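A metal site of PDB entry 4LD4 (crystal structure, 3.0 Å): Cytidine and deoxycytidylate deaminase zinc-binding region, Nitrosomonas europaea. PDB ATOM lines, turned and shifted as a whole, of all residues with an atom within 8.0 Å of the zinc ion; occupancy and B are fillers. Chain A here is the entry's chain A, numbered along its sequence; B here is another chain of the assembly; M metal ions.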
ATOM      1  N   PHE A  50     -35.552 -11.239   3.832  1.00  0.00           N
ATOM      2  CA  PHE A  50     -34.925 -12.125   2.866  1.00  0.00           C
ATOM      3  C   PHE A  50     -35.189 -13.586   3.181  1.00  0.00           C
ATOM      4  O   PHE A  50     -35.148 -13.981   4.345  1.00  0.00           O
ATOM      5  CB  PHE A  50     -33.418 -11.884   2.848  1.00  0.00           C
ATOM      6  CG  PHE A  50     -33.028 -10.485   2.466  1.00  0.00           C
ATOM      7  CD1 PHE A  50     -33.043 -10.085   1.136  1.00  0.00           C
ATOM      8  CD2 PHE A  50     -32.722  -9.540   3.441  1.00  0.00           C
ATOM      9  CE1 PHE A  50     -32.740  -8.780   0.779  1.00  0.00           C
ATOM     10  CE2 PHE A  50     -32.408  -8.225   3.093  1.00  0.00           C
ATOM     11  CZ  PHE A  50     -32.437  -7.844   1.757  1.00  0.00           C
ATOM     12  N   ASN A  68     -33.198 -14.736   6.620  1.00  0.00           N
ATOM     13  CA  ASN A  68     -32.219 -13.935   7.327  1.00  0.00           C
ATOM     14  C   ASN A  68     -32.532 -13.923   8.841  1.00  0.00           C
ATOM     15  O   ASN A  68     -33.606 -13.506   9.276  1.00  0.00           O
ATOM     16  CB  ASN A  68     -32.229 -12.512   6.732  1.00  0.00           C
ATOM     17  CG  ASN A  68     -31.157 -11.602   7.340  1.00  0.00           C
ATOM     18  OD1 ASN A  68     -30.447 -10.898   6.624  1.00  0.00           O
ATOM     19  ND2 ASN A  68     -31.042 -11.610   8.666  1.00  0.00           N
ATOM     20  N   VAL A  70     -29.919 -12.862  10.936  1.00  0.00           N
ATOM     21  CA  VAL A  70     -28.722 -12.169  11.369  1.00  0.00           C
ATOM     22  C   VAL A  70     -28.838 -11.498  12.752  1.00  0.00           C
ATOM     23  O   VAL A  70     -28.132 -11.881  13.686  1.00  0.00           O
ATOM     24  CB  VAL A  70     -28.295 -11.103  10.341  1.00  0.00           C
ATOM     25  CG1 VAL A  70     -27.042 -10.394  10.813  1.00  0.00           C
ATOM     26  CG2 VAL A  70     -28.027 -11.756   9.006  1.00  0.00           C
ATOM     27  N   SER A  76     -23.911 -12.735  11.796  1.00  0.00           N
ATOM     28  CA  SER A  76     -23.850 -12.049  10.517  1.00  0.00           C
ATOM     29  C   SER A  76     -23.880 -13.014   9.319  1.00  0.00           C
ATOM     30  O   SER A  76     -24.369 -12.659   8.232  1.00  0.00           O
ATOM     31  CB  SER A  76     -22.606 -11.149  10.446  1.00  0.00           C
ATOM     32  OG  SER A  76     -21.440 -11.876  10.121  1.00  0.00           O
ATOM     33  N   ALA A  77     -23.394 -14.236   9.518  1.00  0.00           N
ATOM     34  CA  ALA A  77     -23.382 -15.217   8.438  1.00  0.00           C
ATOM     35  C   ALA A  77     -24.730 -15.900   8.204  1.00  0.00           C
ATOM     36  O   ALA A  77     -24.892 -16.631   7.216  1.00  0.00           O
ATOM     37  CB  ALA A  77     -22.315 -16.264   8.716  1.00  0.00           C
ATOM     38  N   ALA A  78     -25.693 -15.692   9.088  1.00  0.00           N
ATOM     39  CA  ALA A  78     -26.994 -16.338   8.936  1.00  0.00           C
ATOM     40  C   ALA A  78     -27.929 -15.703   7.901  1.00  0.00           C
ATOM     41  O   ALA A  78     -29.040 -15.282   8.224  1.00  0.00           O
ATOM     42  CB  ALA A  78     -27.699 -16.439  10.305  1.00  0.00           C
ATOM     43  N   HIS A  79     -27.460 -15.620   6.668  1.00  0.00           N
ATOM     44  CA  HIS A  79     -28.287 -15.069   5.606  1.00  0.00           C
ATOM     45  C   HIS A  79     -29.330 -16.117   5.228  1.00  0.00           C
ATOM     46  O   HIS A  79     -29.373 -17.193   5.816  1.00  0.00           O
ATOM     47  CB  HIS A  79     -27.439 -14.702   4.391  1.00  0.00           C
ATOM     48  CG  HIS A  79     -26.762 -13.372   4.522  1.00  0.00           C
ATOM     49  ND1 HIS A  79     -25.989 -12.834   3.526  1.00  0.00           N
ATOM     50  CD2 HIS A  79     -26.771 -12.464   5.535  1.00  0.00           C
ATOM     51  CE1 HIS A  79     -25.543 -11.648   3.911  1.00  0.00           C
ATOM     52  NE2 HIS A  79     -26.009 -11.399   5.123  1.00  0.00           N
ATOM     53  N   ALA A  80     -30.164 -15.798   4.239  1.00  0.00           N
ATOM     54  CA  ALA A  80     -31.185 -16.736   3.813  1.00  0.00           C
ATOM     55  C   ALA A  80     -30.568 -17.858   2.991  1.00  0.00           C
ATOM     56  O   ALA A  80     -30.895 -19.033   3.191  1.00  0.00           O
ATOM     57  CB  ALA A  80     -32.260 -16.005   3.006  1.00  0.00           C
ATOM     58  N   GLU A  81     -29.654 -17.511   2.081  1.00  0.00           N
ATOM     59  CA  GLU A  81     -29.005 -18.510   1.253  1.00  0.00           C
ATOM     60  C   GLU A  81     -28.120 -19.491   2.023  1.00  0.00           C
ATOM     61  O   GLU A  81     -28.082 -20.687   1.705  1.00  0.00           O
ATOM     62  CB  GLU A  81     -28.159 -17.838   0.176  1.00  0.00           C
ATOM     63  CG  GLU A  81     -28.953 -17.012  -0.817  1.00  0.00           C
ATOM     64  CD  GLU A  81     -29.136 -15.576  -0.374  1.00  0.00           C
ATOM     65  OE1 GLU A  81     -29.207 -15.323   0.855  1.00  0.00           O
ATOM     66  OE2 GLU A  81     -29.239 -14.695  -1.252  1.00  0.00           O
ATOM     67  N   ILE A  82     -27.399 -19.008   3.037  1.00  0.00           N
ATOM     68  CA  ILE A  82     -26.510 -19.858   3.825  1.00  0.00           C
ATOM     69  C   ILE A  82     -27.314 -20.884   4.617  1.00  0.00           C
ATOM     70  O   ILE A  82     -26.915 -22.034   4.740  1.00  0.00           O
ATOM     71  CB  ILE A  82     -25.624 -19.032   4.827  1.00  0.00           C
ATOM     72  CG1 ILE A  82     -24.804 -17.959   4.085  1.00  0.00           C
ATOM     73  CG2 ILE A  82     -24.660 -19.953   5.564  1.00  0.00           C
ATOM     74  CD1 ILE A  82     -23.782 -18.500   3.100  1.00  0.00           C
ATOM     75  N   ALA A 111     -34.046 -12.197  -3.355  1.00  0.00           N
ATOM     76  CA  ALA A 111     -33.217 -11.100  -3.881  1.00  0.00           C
ATOM     77  C   ALA A 111     -31.859 -11.591  -4.376  1.00  0.00           C
ATOM     78  O   ALA A 111     -31.300 -12.539  -3.839  1.00  0.00           O
ATOM     79  CB  ALA A 111     -33.015 -10.042  -2.802  1.00  0.00           C
ATOM     80  N   GLU A 112     -31.339 -10.936  -5.404  1.00  0.00           N
ATOM     81  CA  GLU A 112     -30.035 -11.309  -5.943  1.00  0.00           C
ATOM     82  C   GLU A 112     -29.071 -11.426  -4.774  1.00  0.00           C
ATOM     83  O   GLU A 112     -28.972 -10.519  -3.951  1.00  0.00           O
ATOM     84  CB  GLU A 112     -29.576 -10.257  -6.947  1.00  0.00           C
ATOM     85  CG  GLU A 112     -30.401 -10.289  -8.219  1.00  0.00           C
ATOM     86  CD  GLU A 112     -29.995  -9.226  -9.217  1.00  0.00           C
ATOM     87  OE1 GLU A 112     -30.544  -9.233 -10.327  1.00  0.00           O
ATOM     88  OE2 GLU A 112     -29.135  -8.397  -8.877  1.00  0.00           O
ATOM     89  N   PRO A 113     -28.349 -12.555  -4.691  1.00  0.00           N
ATOM     90  CA  PRO A 113     -27.383 -12.850  -3.628  1.00  0.00           C
ATOM     91  C   PRO A 113     -26.267 -11.841  -3.396  1.00  0.00           C
ATOM     92  O   PRO A 113     -25.788 -11.194  -4.339  1.00  0.00           O
ATOM     93  CB  PRO A 113     -26.854 -14.228  -4.023  1.00  0.00           C
ATOM     94  CG  PRO A 113     -26.837 -14.157  -5.496  1.00  0.00           C
ATOM     95  CD  PRO A 113     -28.168 -13.494  -5.821  1.00  0.00           C
ATOM     96  N   CYS A 114     -25.855 -11.704  -2.140  1.00  0.00           N
ATOM     97  CA  CYS A 114     -24.793 -10.770  -1.805  1.00  0.00           C
ATOM     98  C   CYS A 114     -23.459 -11.452  -2.114  1.00  0.00           C
ATOM     99  O   CYS A 114     -23.421 -12.607  -2.530  1.00  0.00           O
ATOM    100  CB  CYS A 114     -24.863 -10.352  -0.327  1.00  0.00           C
ATOM    101  SG  CYS A 114     -24.181 -11.493   0.892  1.00  0.00           S
ATOM    102  N   VAL A 115     -22.360 -10.722  -1.911  1.00  0.00           N
ATOM    103  CA  VAL A 115     -21.037 -11.243  -2.196  1.00  0.00           C
ATOM    104  C   VAL A 115     -20.722 -12.508  -1.395  1.00  0.00           C
ATOM    105  O   VAL A 115     -20.244 -13.486  -1.956  1.00  0.00           O
ATOM    106  CB  VAL A 115     -19.963 -10.153  -1.943  1.00  0.00           C
ATOM    107  CG1 VAL A 115     -19.922  -9.781  -0.475  1.00  0.00           C
ATOM    108  CG2 VAL A 115     -18.612 -10.632  -2.445  1.00  0.00           C
ATOM    109  N   MET A 116     -21.005 -12.487  -0.092  1.00  0.00           N
ATOM    110  CA  MET A 116     -20.758 -13.663   0.754  1.00  0.00           C
ATOM    111  C   MET A 116     -21.475 -14.874   0.186  1.00  0.00           C
ATOM    112  O   MET A 116     -20.849 -15.882  -0.159  1.00  0.00           O
ATOM    113  CB  MET A 116     -21.240 -13.408   2.173  1.00  0.00           C
ATOM    114  CG  MET A 116     -21.315 -14.668   3.044  1.00  0.00           C
ATOM    115  SD  MET A 116     -22.269 -14.418   4.575  1.00  0.00           S
ATOM    116  CE  MET A 116     -21.048 -14.722   5.777  1.00  0.00           C
ATOM    117  N   CYS A 117     -22.790 -14.768   0.082  1.00  0.00           N
ATOM    118  CA  CYS A 117     -23.615 -15.860  -0.430  1.00  0.00           C
ATOM    119  C   CYS A 117     -23.312 -16.188  -1.889  1.00  0.00           C
ATOM    120  O   CYS A 117     -23.495 -17.330  -2.315  1.00  0.00           O
ATOM    121  CB  CYS A 117     -25.095 -15.532  -0.269  1.00  0.00           C
ATOM    122  SG  CYS A 117     -25.555 -15.288   1.465  1.00  0.00           S
ATOM    123  N   PHE A 118     -22.835 -15.205  -2.642  1.00  0.00           N
ATOM    124  CA  PHE A 118     -22.495 -15.403  -4.052  1.00  0.00           C
ATOM    125  C   PHE A 118     -21.543 -16.586  -4.208  1.00  0.00           C
ATOM    126  O   PHE A 118     -21.693 -17.415  -5.113  1.00  0.00           O
ATOM    127  CB  PHE A 118     -21.839 -14.157  -4.629  1.00  0.00           C
ATOM    128  CG  PHE A 118     -20.966 -14.421  -5.834  1.00  0.00           C
ATOM    129  CD1 PHE A 118     -21.520 -14.882  -7.036  1.00  0.00           C
ATOM    130  CD2 PHE A 118     -19.598 -14.170  -5.786  1.00  0.00           C
ATOM    131  CE1 PHE A 118     -20.708 -15.086  -8.147  1.00  0.00           C
ATOM    132  CE2 PHE A 118     -18.785 -14.375  -6.897  1.00  0.00           C
ATOM    133  CZ  PHE A 118     -19.343 -14.827  -8.081  1.00  0.00           C
ATOM    134  N   ALA A 120     -20.968 -18.689  -1.646  1.00  0.00           N
ATOM    135  CA  ALA A 120     -21.639 -19.760  -0.929  1.00  0.00           C
ATOM    136  C   ALA A 120     -22.394 -20.624  -1.928  1.00  0.00           C
ATOM    137  O   ALA A 120     -22.467 -21.845  -1.775  1.00  0.00           O
ATOM    138  CB  ALA A 120     -22.607 -19.182   0.084  1.00  0.00           C
ATOM    139  N   ASP A 144     -26.613  -3.781   1.882  1.00  0.00           N
ATOM    140  CA  ASP A 144     -25.522  -3.763   0.942  1.00  0.00           C
ATOM    141  C   ASP A 144     -25.335  -5.137   0.312  1.00  0.00           C
ATOM    142  O   ASP A 144     -25.398  -6.153   1.003  1.00  0.00           O
ATOM    143  CB  ASP A 144     -24.244  -3.366   1.691  1.00  0.00           C
ATOM    144  CG  ASP A 144     -23.154  -2.899   0.764  1.00  0.00           C
ATOM    145  OD1 ASP A 144     -22.017  -2.689   1.243  1.00  0.00           O
ATOM    146  OD2 ASP A 144     -23.445  -2.745  -0.444  1.00  0.00           O
ATOM    147  N   GLU A 145     -25.097  -5.179  -1.002  1.00  0.00           N
ATOM    148  CA  GLU A 145     -24.870  -6.447  -1.674  1.00  0.00           C
ATOM    149  C   GLU A 145     -23.407  -6.850  -1.487  1.00  0.00           C
ATOM    150  O   GLU A 145     -23.064  -8.024  -1.568  1.00  0.00           O
ATOM    151  CB  GLU A 145     -25.200  -6.354  -3.165  1.00  0.00           C
ATOM    152  CG  GLU A 145     -26.677  -6.346  -3.473  1.00  0.00           C
ATOM    153  CD  GLU A 145     -27.369  -7.620  -3.036  1.00  0.00           C
ATOM    154  OE1 GLU A 145     -27.212  -8.009  -1.860  1.00  0.00           O
ATOM    155  OE2 GLU A 145     -28.065  -8.237  -3.868  1.00  0.00           O
ATOM    156  N   TRP B 123     -19.018  -8.496   6.684  1.00  0.00           N
ATOM    157  CA  TRP B 123     -20.225  -8.358   7.502  1.00  0.00           C
ATOM    158  C   TRP B 123     -20.011  -8.673   8.983  1.00  0.00           C
ATOM    159  O   TRP B 123     -20.914  -8.461   9.789  1.00  0.00           O
ATOM    160  CB  TRP B 123     -21.332  -9.303   7.004  1.00  0.00           C
ATOM    161  CG  TRP B 123     -21.621  -9.273   5.539  1.00  0.00           C
ATOM    162  CD1 TRP B 123     -21.864 -10.348   4.730  1.00  0.00           C
ATOM    163  CD2 TRP B 123     -21.734  -8.108   4.706  1.00  0.00           C
ATOM    164  NE1 TRP B 123     -22.105  -9.926   3.441  1.00  0.00           N
ATOM    165  CE2 TRP B 123     -22.036  -8.568   3.402  1.00  0.00           C
ATOM    166  CE3 TRP B 123     -21.602  -6.739   4.935  1.00  0.00           C
ATOM    167  CZ2 TRP B 123     -22.209  -7.683   2.315  1.00  0.00           C
ATOM    168  CZ3 TRP B 123     -21.783  -5.868   3.865  1.00  0.00           C
ATOM    169  CH2 TRP B 123     -22.083  -6.347   2.570  1.00  0.00           C
HETATM  170 ZN    ZN M   1     -25.965 -12.961   1.404  1.00  0.00          ZN
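Within 4 Å of the zinc ion: His 79, Cys 114 and Cys 117. The nearest printed residue that does not touch the zinc ion is Glu 81 (4.05 Å).
SG of Cys 114 lies close to N of Met 116. SG of Cys 117 lies close to OE1 of Glu 81. The side-chain sulfur (SG) of Cys 114 lies close to the indole nitrogen (NE1) of Trp 123 of chain B (3.6 Å).
ND1 of His 79 is bound to the zinc ion (2.1 Å). The zinc ion is bound by SG of Cys 117. SG of Cys 114 is bound to the zinc ion, 2.4 Å away. The zinc ion has three donor atoms within binding distance.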
